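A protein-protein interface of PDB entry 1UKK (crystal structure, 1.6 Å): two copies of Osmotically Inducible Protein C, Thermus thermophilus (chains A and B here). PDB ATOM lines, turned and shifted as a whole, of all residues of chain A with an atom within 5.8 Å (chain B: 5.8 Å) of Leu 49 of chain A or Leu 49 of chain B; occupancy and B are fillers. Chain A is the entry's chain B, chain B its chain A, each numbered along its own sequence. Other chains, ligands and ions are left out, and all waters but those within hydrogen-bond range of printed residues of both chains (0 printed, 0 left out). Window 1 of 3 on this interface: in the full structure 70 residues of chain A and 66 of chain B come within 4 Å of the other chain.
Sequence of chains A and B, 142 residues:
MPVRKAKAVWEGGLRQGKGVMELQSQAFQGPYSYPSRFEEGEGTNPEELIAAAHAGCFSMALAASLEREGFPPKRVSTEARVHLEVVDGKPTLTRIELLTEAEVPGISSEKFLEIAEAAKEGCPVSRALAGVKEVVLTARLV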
ATOM      1  N   MET A  21     -17.166 -14.724 -31.271  1.00  0.00           N
ATOM      2  CA  MET A  21     -17.472 -15.132 -29.878  1.00  0.00           C
ATOM      3  C   MET A  21     -16.415 -14.516 -28.997  1.00  0.00           C
ATOM      4  O   MET A  21     -15.251 -14.520 -29.346  1.00  0.00           O
ATOM      5  CB  MET A  21     -17.428 -16.649 -29.750  1.00  0.00           C
ATOM      6  CG  MET A  21     -18.701 -17.391 -30.197  1.00  0.00           C
ATOM      7  SD  MET A  21     -18.584 -19.259 -30.335  1.00  0.00           S
ATOM      8  CE  MET A  21     -17.335 -19.322 -31.857  1.00  0.00           C
ATOM      9  N   LEU A  23     -14.990 -13.974 -24.833  1.00  0.00           N
ATOM     10  CA  LEU A  23     -15.061 -14.343 -23.404  1.00  0.00           C
ATOM     11  C   LEU A  23     -15.087 -13.108 -22.459  1.00  0.00           C
ATOM     12  O   LEU A  23     -14.520 -12.051 -22.841  1.00  0.00           O
ATOM     13  CB  LEU A  23     -13.874 -15.240 -23.114  1.00  0.00           C
ATOM     14  CG  LEU A  23     -13.885 -16.600 -23.840  1.00  0.00           C
ATOM     15  CD1 LEU A  23     -12.852 -17.515 -23.243  1.00  0.00           C
ATOM     16  CD2 LEU A  23     -15.212 -17.313 -23.780  1.00  0.00           C
ATOM     17  N   PHE A  28     -10.272 -13.077 -25.581  1.00  0.00           N
ATOM     18  CA  PHE A  28     -10.327 -13.985 -26.707  1.00  0.00           C
ATOM     19  C   PHE A  28     -11.422 -13.512 -27.638  1.00  0.00           C
ATOM     20  O   PHE A  28     -12.488 -13.187 -27.189  1.00  0.00           O
ATOM     21  CB  PHE A  28     -10.621 -15.363 -26.182  1.00  0.00           C
ATOM     22  CG  PHE A  28     -11.184 -16.341 -27.198  1.00  0.00           C
ATOM     23  CD1 PHE A  28     -10.349 -17.127 -27.939  1.00  0.00           C
ATOM     24  CD2 PHE A  28     -12.551 -16.506 -27.323  1.00  0.00           C
ATOM     25  CE1 PHE A  28     -10.864 -18.037 -28.816  1.00  0.00           C
ATOM     26  CE2 PHE A  28     -13.075 -17.441 -28.182  1.00  0.00           C
ATOM     27  CZ  PHE A  28     -12.239 -18.193 -28.929  1.00  0.00           C
ATOM     28  N   THR A  44     -13.096 -20.554 -35.820  1.00  0.00           N
ATOM     29  CA  THR A  44     -13.491 -21.542 -34.840  1.00  0.00           C
ATOM     30  C   THR A  44     -15.026 -21.668 -34.931  1.00  0.00           C
ATOM     31  O   THR A  44     -15.638 -21.368 -36.006  1.00  0.00           O
ATOM     32  CB  THR A  44     -12.957 -21.163 -33.436  1.00  0.00           C
ATOM     33  OG1 THR A  44     -13.424 -22.131 -32.486  1.00  0.00           O
ATOM     34  CG2 THR A  44     -13.469 -19.772 -32.990  1.00  0.00           C
ATOM     35  N   ASN A  45     -15.652 -22.215 -33.909  1.00  0.00           N
ATOM     36  CA  ASN A  45     -17.093 -22.545 -34.010  1.00  0.00           C
ATOM     37  C   ASN A  45     -17.581 -22.921 -32.646  1.00  0.00           C
ATOM     38  O   ASN A  45     -16.758 -23.194 -31.727  1.00  0.00           O
ATOM     39  CB  ASN A  45     -17.371 -23.724 -35.007  1.00  0.00           C
ATOM     40  CG  ASN A  45     -16.381 -24.812 -34.836  1.00  0.00           C
ATOM     41  OD1 ASN A  45     -16.456 -25.531 -33.857  1.00  0.00           O
ATOM     42  ND2 ASN A  45     -15.480 -24.966 -35.788  1.00  0.00           N
ATOM     43  N   PRO A  46     -18.912 -22.895 -32.419  1.00  0.00           N
ATOM     44  CA  PRO A  46     -19.427 -23.269 -31.122  1.00  0.00           C
ATOM     45  C   PRO A  46     -18.982 -24.661 -30.644  1.00  0.00           C
ATOM     46  O   PRO A  46     -18.747 -24.925 -29.470  1.00  0.00           O
ATOM     47  CB  PRO A  46     -20.966 -23.195 -31.307  1.00  0.00           C
ATOM     48  CG  PRO A  46     -21.126 -22.133 -32.357  1.00  0.00           C
ATOM     49  CD  PRO A  46     -19.957 -22.331 -33.299  1.00  0.00           C
ATOM     50  N   GLU A  47     -18.857 -25.587 -31.581  1.00  0.00           N
ATOM     51  CA  GLU A  47     -18.528 -26.973 -31.246  1.00  0.00           C
ATOM     52  C   GLU A  47     -17.093 -27.095 -30.661  1.00  0.00           C
ATOM     53  O   GLU A  47     -16.864 -27.917 -29.738  1.00  0.00           O
ATOM     54  CB  GLU A  47     -18.685 -27.806 -32.507  1.00  0.00           C
ATOM     55  CG  GLU A  47     -20.137 -28.058 -32.910  1.00  0.00           C
ATOM     56  CD  GLU A  47     -20.873 -26.797 -33.414  1.00  0.00           C
ATOM     57  OE1 GLU A  47     -20.267 -25.974 -34.157  1.00  0.00           O
ATOM     58  OE2 GLU A  47     -22.051 -26.665 -33.065  1.00  0.00           O
ATOM     59  N   GLU A  48     -16.179 -26.281 -31.134  1.00  0.00           N
ATOM     60  CA  GLU A  48     -14.811 -26.226 -30.602  1.00  0.00           C
ATOM     61  C   GLU A  48     -14.807 -25.752 -29.150  1.00  0.00           C
ATOM     62  O   GLU A  48     -14.132 -26.338 -28.311  1.00  0.00           O
ATOM     63  CB  GLU A  48     -13.880 -25.411 -31.471  1.00  0.00           C
ATOM     64  CG  GLU A  48     -13.434 -26.223 -32.642  1.00  0.00           C
ATOM     65  CD  GLU A  48     -12.562 -25.472 -33.607  1.00  0.00           C
ATOM     66  OE1 GLU A  48     -11.995 -24.347 -33.261  1.00  0.00           O
ATOM     67  OE2 GLU A  48     -12.494 -26.053 -34.756  1.00  0.00           O
ATOM     68  N   LEU A  49     -15.608 -24.721 -28.860  1.00  0.00           N
ATOM     69  CA  LEU A  49     -15.706 -24.223 -27.494  1.00  0.00           C
ATOM     70  C   LEU A  49     -16.377 -25.294 -26.607  1.00  0.00           C
ATOM     71  O   LEU A  49     -15.989 -25.494 -25.448  1.00  0.00           O
ATOM     72  CB  LEU A  49     -16.486 -22.933 -27.488  1.00  0.00           C
ATOM     73  CG  LEU A  49     -15.746 -21.606 -27.792  1.00  0.00           C
ATOM     74  CD1 LEU A  49     -14.729 -21.256 -26.712  1.00  0.00           C
ATOM     75  CD2 LEU A  49     -14.988 -21.628 -29.086  1.00  0.00           C
ATOM     76  N   ILE A  50     -17.419 -26.014 -27.045  1.00  0.00           N
ATOM     77  CA  ILE A  50     -17.997 -27.095 -26.294  1.00  0.00           C
ATOM     78  C   ILE A  50     -16.947 -28.217 -26.043  1.00  0.00           C
ATOM     79  O   ILE A  50     -16.880 -28.769 -24.946  1.00  0.00           O
ATOM     80  CB  ILE A  50     -19.193 -27.701 -27.085  1.00  0.00           C
ATOM     81  CG1 ILE A  50     -20.332 -26.666 -27.208  1.00  0.00           C
ATOM     82  CG2 ILE A  50     -19.661 -28.968 -26.402  1.00  0.00           C
ATOM     83  CD1 ILE A  50     -20.856 -26.178 -25.840  1.00  0.00           C
ATOM     84  N   ALA A  51     -16.220 -28.582 -27.067  1.00  0.00           N
ATOM     85  CA  ALA A  51     -15.097 -29.543 -26.914  1.00  0.00           C
ATOM     86  C   ALA A  51     -14.137 -29.153 -25.764  1.00  0.00           C
ATOM     87  O   ALA A  51     -13.857 -29.981 -24.859  1.00  0.00           O
ATOM     88  CB  ALA A  51     -14.303 -29.727 -28.239  1.00  0.00           C
ATOM     89  N   ALA A  52     -13.715 -27.905 -25.771  1.00  0.00           N
ATOM     90  CA  ALA A  52     -12.790 -27.388 -24.730  1.00  0.00           C
ATOM     91  C   ALA A  52     -13.398 -27.461 -23.366  1.00  0.00           C
ATOM     92  O   ALA A  52     -12.750 -27.876 -22.415  1.00  0.00           O
ATOM     93  CB  ALA A  52     -12.399 -26.028 -25.006  1.00  0.00           C
ATOM     94  N   ALA A  53     -14.672 -27.079 -23.258  1.00  0.00           N
ATOM     95  CA  ALA A  53     -15.400 -27.149 -21.978  1.00  0.00           C
ATOM     96  C   ALA A  53     -15.498 -28.560 -21.477  1.00  0.00           C
ATOM     97  O   ALA A  53     -15.321 -28.870 -20.304  1.00  0.00           O
ATOM     98  CB  ALA A  53     -16.856 -26.591 -22.132  1.00  0.00           C
ATOM     99  N   HIS A  54     -15.852 -29.483 -22.358  1.00  0.00           N
ATOM    100  CA  HIS A  54     -16.001 -30.831 -21.923  1.00  0.00           C
ATOM    101  C   HIS A  54     -14.677 -31.485 -21.536  1.00  0.00           C
ATOM    102  O   HIS A  54     -14.609 -32.220 -20.496  1.00  0.00           O
ATOM    103  CB  HIS A  54     -16.657 -31.593 -23.035  1.00  0.00           C
ATOM    104  CG  HIS A  54     -17.368 -32.804 -22.559  1.00  0.00           C
ATOM    105  ND1 HIS A  54     -17.951 -33.695 -23.427  1.00  0.00           N
ATOM    106  CD2 HIS A  54     -17.601 -33.284 -21.313  1.00  0.00           C
ATOM    107  CE1 HIS A  54     -18.486 -34.690 -22.738  1.00  0.00           C
ATOM    108  NE2 HIS A  54     -18.303 -34.461 -21.454  1.00  0.00           N
ATOM    109  N   MET B  21      -7.403 -25.169 -20.638  1.00  0.00           N
ATOM    110  CA  MET B  21      -8.157 -25.619 -21.804  1.00  0.00           C
ATOM    111  C   MET B  21      -7.521 -24.915 -23.009  1.00  0.00           C
ATOM    112  O   MET B  21      -7.188 -23.734 -22.965  1.00  0.00           O
ATOM    113  CB  MET B  21      -9.646 -25.252 -21.694  1.00  0.00           C
ATOM    114  CG  MET B  21     -10.462 -26.061 -20.700  1.00  0.00           C
ATOM    115  SD  MET B  21     -12.171 -25.307 -20.262  1.00  0.00           S
ATOM    116  CE  MET B  21     -11.643 -23.834 -19.146  1.00  0.00           C
ATOM    117  N   LEU B  23      -7.553 -24.318 -27.361  1.00  0.00           N
ATOM    118  CA  LEU B  23      -7.945 -24.393 -28.746  1.00  0.00           C
ATOM    119  C   LEU B  23      -6.647 -24.028 -29.490  1.00  0.00           C
ATOM    120  O   LEU B  23      -6.386 -22.836 -29.739  1.00  0.00           O
ATOM    121  CB  LEU B  23      -8.976 -23.348 -29.082  1.00  0.00           C
ATOM    122  CG  LEU B  23     -10.314 -23.126 -28.359  1.00  0.00           C
ATOM    123  CD1 LEU B  23     -11.046 -22.051 -29.111  1.00  0.00           C
ATOM    124  CD2 LEU B  23     -11.187 -24.295 -28.293  1.00  0.00           C
ATOM    125  N   PHE B  28      -5.365 -20.198 -28.209  1.00  0.00           N
ATOM    126  CA  PHE B  28      -6.065 -19.938 -26.958  1.00  0.00           C
ATOM    127  C   PHE B  28      -5.698 -20.950 -25.883  1.00  0.00           C
ATOM    128  O   PHE B  28      -5.777 -22.166 -26.091  1.00  0.00           O
ATOM    129  CB  PHE B  28      -7.576 -19.988 -27.197  1.00  0.00           C
ATOM    130  CG  PHE B  28      -8.398 -19.935 -25.936  1.00  0.00           C
ATOM    131  CD1 PHE B  28      -8.658 -18.719 -25.351  1.00  0.00           C
ATOM    132  CD2 PHE B  28      -8.904 -21.084 -25.370  1.00  0.00           C
ATOM    133  CE1 PHE B  28      -9.415 -18.651 -24.150  1.00  0.00           C
ATOM    134  CE2 PHE B  28      -9.648 -21.016 -24.169  1.00  0.00           C
ATOM    135  CZ  PHE B  28      -9.904 -19.811 -23.595  1.00  0.00           C
ATOM    136  N   THR B  44     -10.604 -18.733 -16.268  1.00  0.00           N
ATOM    137  CA  THR B  44     -11.851 -18.975 -16.906  1.00  0.00           C
ATOM    138  C   THR B  44     -12.371 -20.347 -16.350  1.00  0.00           C
ATOM    139  O   THR B  44     -11.925 -20.830 -15.259  1.00  0.00           O
ATOM    140  CB  THR B  44     -11.671 -18.965 -18.427  1.00  0.00           C
ATOM    141  OG1 THR B  44     -12.950 -19.271 -19.087  1.00  0.00           O
ATOM    142  CG2 THR B  44     -10.772 -20.095 -18.921  1.00  0.00           C
ATOM    143  N   ASN B  45     -13.289 -20.990 -17.066  1.00  0.00           N
ATOM    144  CA  ASN B  45     -13.900 -22.235 -16.605  1.00  0.00           C
ATOM    145  C   ASN B  45     -14.726 -22.880 -17.721  1.00  0.00           C
ATOM    146  O   ASN B  45     -14.989 -22.174 -18.756  1.00  0.00           O
ATOM    147  CB  ASN B  45     -14.808 -22.008 -15.395  1.00  0.00           C
ATOM    148  CG  ASN B  45     -15.608 -20.730 -15.544  1.00  0.00           C
ATOM    149  OD1 ASN B  45     -16.511 -20.683 -16.395  1.00  0.00           O
ATOM    150  ND2 ASN B  45     -15.296 -19.688 -14.707  1.00  0.00           N
ATOM    151  N   PRO B  46     -15.095 -24.155 -17.610  1.00  0.00           N
ATOM    152  CA  PRO B  46     -15.947 -24.803 -18.638  1.00  0.00           C
ATOM    153  C   PRO B  46     -17.237 -24.017 -18.929  1.00  0.00           C
ATOM    154  O   PRO B  46     -17.678 -23.909 -20.076  1.00  0.00           O
ATOM    155  CB  PRO B  46     -16.221 -26.220 -18.072  1.00  0.00           C
ATOM    156  CG  PRO B  46     -14.993 -26.442 -17.253  1.00  0.00           C
ATOM    157  CD  PRO B  46     -14.617 -25.110 -16.590  1.00  0.00           C
ATOM    158  N   GLU B  47     -17.793 -23.416 -17.883  1.00  0.00           N
ATOM    159  CA  GLU B  47     -19.076 -22.749 -17.981  1.00  0.00           C
ATOM    160  C   GLU B  47     -19.030 -21.490 -18.883  1.00  0.00           C
ATOM    161  O   GLU B  47     -19.970 -21.290 -19.661  1.00  0.00           O
ATOM    162  CB  GLU B  47     -19.602 -22.402 -16.588  1.00  0.00           C
ATOM    163  CG  GLU B  47     -20.108 -23.585 -15.717  1.00  0.00           C
ATOM    164  CD  GLU B  47     -19.010 -24.595 -15.305  1.00  0.00           C
ATOM    165  OE1 GLU B  47     -17.848 -24.145 -14.984  1.00  0.00           O
ATOM    166  OE2 GLU B  47     -19.258 -25.791 -15.414  1.00  0.00           O
ATOM    167  N   GLU B  48     -17.926 -20.748 -18.834  1.00  0.00           N
ATOM    168  CA  GLU B  48     -17.677 -19.569 -19.653  1.00  0.00           C
ATOM    169  C   GLU B  48     -17.599 -19.991 -21.129  1.00  0.00           C
ATOM    170  O   GLU B  48     -18.159 -19.341 -21.989  1.00  0.00           O
ATOM    171  CB  GLU B  48     -16.461 -18.815 -19.192  1.00  0.00           C
ATOM    172  CG  GLU B  48     -16.398 -17.444 -19.838  1.00  0.00           C
ATOM    173  CD  GLU B  48     -15.218 -16.602 -19.399  1.00  0.00           C
ATOM    174  OE1 GLU B  48     -14.398 -17.056 -18.580  1.00  0.00           O
ATOM    175  OE2 GLU B  48     -15.150 -15.478 -19.869  1.00  0.00           O
ATOM    176  N   LEU B  49     -16.942 -21.109 -21.409  1.00  0.00           N
ATOM    177  CA  LEU B  49     -16.809 -21.574 -22.772  1.00  0.00           C
ATOM    178  C   LEU B  49     -18.166 -22.065 -23.310  1.00  0.00           C
ATOM    179  O   LEU B  49     -18.472 -21.871 -24.491  1.00  0.00           O
ATOM    180  CB  LEU B  49     -15.774 -22.692 -22.832  1.00  0.00           C
ATOM    181  CG  LEU B  49     -14.346 -22.173 -22.969  1.00  0.00           C
ATOM    182  CD1 LEU B  49     -13.931 -21.217 -21.989  1.00  0.00           C
ATOM    183  CD2 LEU B  49     -13.364 -23.246 -22.943  1.00  0.00           C
ATOM    184  N   ILE B  50     -18.973 -22.729 -22.500  1.00  0.00           N
ATOM    185  CA  ILE B  50     -20.322 -23.139 -22.878  1.00  0.00           C
ATOM    186  C   ILE B  50     -21.155 -21.861 -23.169  1.00  0.00           C
ATOM    187  O   ILE B  50     -21.920 -21.814 -24.131  1.00  0.00           O
ATOM    188  CB  ILE B  50     -21.026 -23.938 -21.720  1.00  0.00           C
ATOM    189  CG1 ILE B  50     -20.351 -25.301 -21.505  1.00  0.00           C
ATOM    190  CG2 ILE B  50     -22.506 -24.114 -22.009  1.00  0.00           C
ATOM    191  CD1 ILE B  50     -20.336 -26.129 -22.734  1.00  0.00           C
ATOM    192  N   ALA B  51     -21.046 -20.870 -22.310  1.00  0.00           N
ATOM    193  CA  ALA B  51     -21.781 -19.620 -22.549  1.00  0.00           C
ATOM    194  C   ALA B  51     -21.446 -19.042 -23.963  1.00  0.00           C
ATOM    195  O   ALA B  51     -22.328 -18.653 -24.761  1.00  0.00           O
ATOM    196  CB  ALA B  51     -21.473 -18.547 -21.466  1.00  0.00           C
ATOM    197  N   ALA B  52     -20.168 -19.028 -24.294  1.00  0.00           N
ATOM    198  CA  ALA B  52     -19.701 -18.494 -25.596  1.00  0.00           C
ATOM    199  C   ALA B  52     -20.242 -19.318 -26.764  1.00  0.00           C
ATOM    200  O   ALA B  52     -20.690 -18.772 -27.760  1.00  0.00           O
ATOM    201  CB  ALA B  52     -18.223 -18.486 -25.653  1.00  0.00           C
ATOM    202  N   ALA B  53     -20.188 -20.633 -26.613  1.00  0.00           N
ATOM    203  CA  ALA B  53     -20.798 -21.582 -27.575  1.00  0.00           C
ATOM    204  C   ALA B  53     -22.272 -21.362 -27.777  1.00  0.00           C
ATOM    205  O   ALA B  53     -22.757 -21.273 -28.901  1.00  0.00           O
ATOM    206  CB  ALA B  53     -20.594 -22.990 -27.136  1.00  0.00           C
ATOM    207  N   HIS B  54     -23.006 -21.187 -26.695  1.00  0.00           N
ATOM    208  CA  HIS B  54     -24.408 -20.980 -26.854  1.00  0.00           C
ATOM    209  C   HIS B  54     -24.754 -19.632 -27.455  1.00  0.00           C
ATOM    210  O   HIS B  54     -25.663 -19.555 -28.334  1.00  0.00           O
ATOM    211  CB  HIS B  54     -25.030 -21.108 -25.463  1.00  0.00           C
ATOM    212  CG  HIS B  54     -26.461 -21.545 -25.469  1.00  0.00           C
ATOM    213  ND1 HIS B  54     -27.158 -21.802 -24.310  1.00  0.00           N
ATOM    214  CD2 HIS B  54     -27.331 -21.782 -26.488  1.00  0.00           C
ATOM    215  CE1 HIS B  54     -28.399 -22.145 -24.613  1.00  0.00           C
ATOM    216  NE2 HIS B  54     -28.526 -22.168 -25.926  1.00  0.00           N
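Among the printed residues, merely in contact across the chains: Leu 23 of chain A with Phe 28 of chain B, Leu 23 of chain A with Glu 48 of chain B, Leu 23 of chain A with Ala 52 of chain B, Phe 28 of chain A with Phe 28 of chain B, Pro 46 of chain A with Ala 53 of chain B, Glu 48 of chain A with Leu 23 of chain B, Leu 49 of chain A with Leu 23 of chain B, Leu 49 of chain A with Leu 49 of chain B, Ile 50 of chain A with Ile 50 of chain B, Ile 50 of chain A with Ala 53 of chain B, Ala 52 of chain A with Leu 23 of chain B, Ala 52 of chain A with Leu 49 of chain B, Ala 53 of chain A with Pro 46 of chain B and Ala 53 of chain A with Ile 50 of chain B.
O of Ala 52 of chain B sits close to SD of Met 21 of chain A (3.4 Å).
O of Ala 52 of chain A sits close to SD of Met 21 of chain B (3.4 Å).
Of the 14 printed residues of chain B, 9 touch a printed residue of chain A.
Hydrophobic or aromatic side chains of chain B that line the printed part of chain A: Met 21, Leu 23, Phe 28, Pro 46, Leu 49, Ile 50, Ala 52 and Ala 53.
Hydrophobic or aromatic side chains of chain A within 4 Å of the printed part of chain B: Met 21, Leu 23, Phe 28, Pro 46, Leu 49, Ile 50, Ala 52 and Ala 53.
Printed residues of chain B within 4 Å of Met 21 of chain A: Ala 52.
Printed residues of chain B within 4 Å of Phe 28 of chain A: Phe 28 (3.5 Å).
Of the printed residues of chain A, Pro 46 of chain B touches Ala 53 (3.5 Å).
Leu 49 of chain B touches just these residues of chain A: Leu 49 and Ala 52.
The backbone NH of Leu 23 of chain B lies within hydrogen-bond range of the backbone carbonyl oxygen of Phe 28 of chain B (3.1 Å).
The side-chain hydroxyl of Thr 44 of chain B sits at hydrogen-bond distance from the side-chain carboxylate of Glu 48 of chain B (2.7 Å).
OD1 of Asn 45 of chain B sits at hydrogen-bond distance from N of Glu 48 of chain B.
OG1 of Thr 44 of chain A is in hydrogen-bond range of OE1 of Glu 48 of chain A, at 2.7 Å.
The side-chain amide oxygen (OD1) of Asn 45 of chain A lies within hydrogen-bond range of the backbone NH (N) of Glu 48 of chain A.
Leu 23 of chain A touches Phe 28 of chain B, but with the chains exchanged Phe 28 of chain A does not touch Leu 23 of chain B (4.03 Å).
Leu 23 of chain A touches Glu 48 of chain B, and with the chains exchanged Glu 48 of chain A touches Leu 23 of chain B.
Leu 23 of chain A touches Ala 52 of chain B, and with the chains exchanged Ala 52 of chain A touches Leu 23 of chain B.
Leu 49 of chain A touches Leu 23 of chain B, but with the chains exchanged Leu 23 of chain A does not touch Leu 49 of chain B (4.1 Å).
Positions printed for both chains: 21, 23, 28, 44, 45, 46, 47, 48, 49, 50, 51, 52, 53 and 54.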
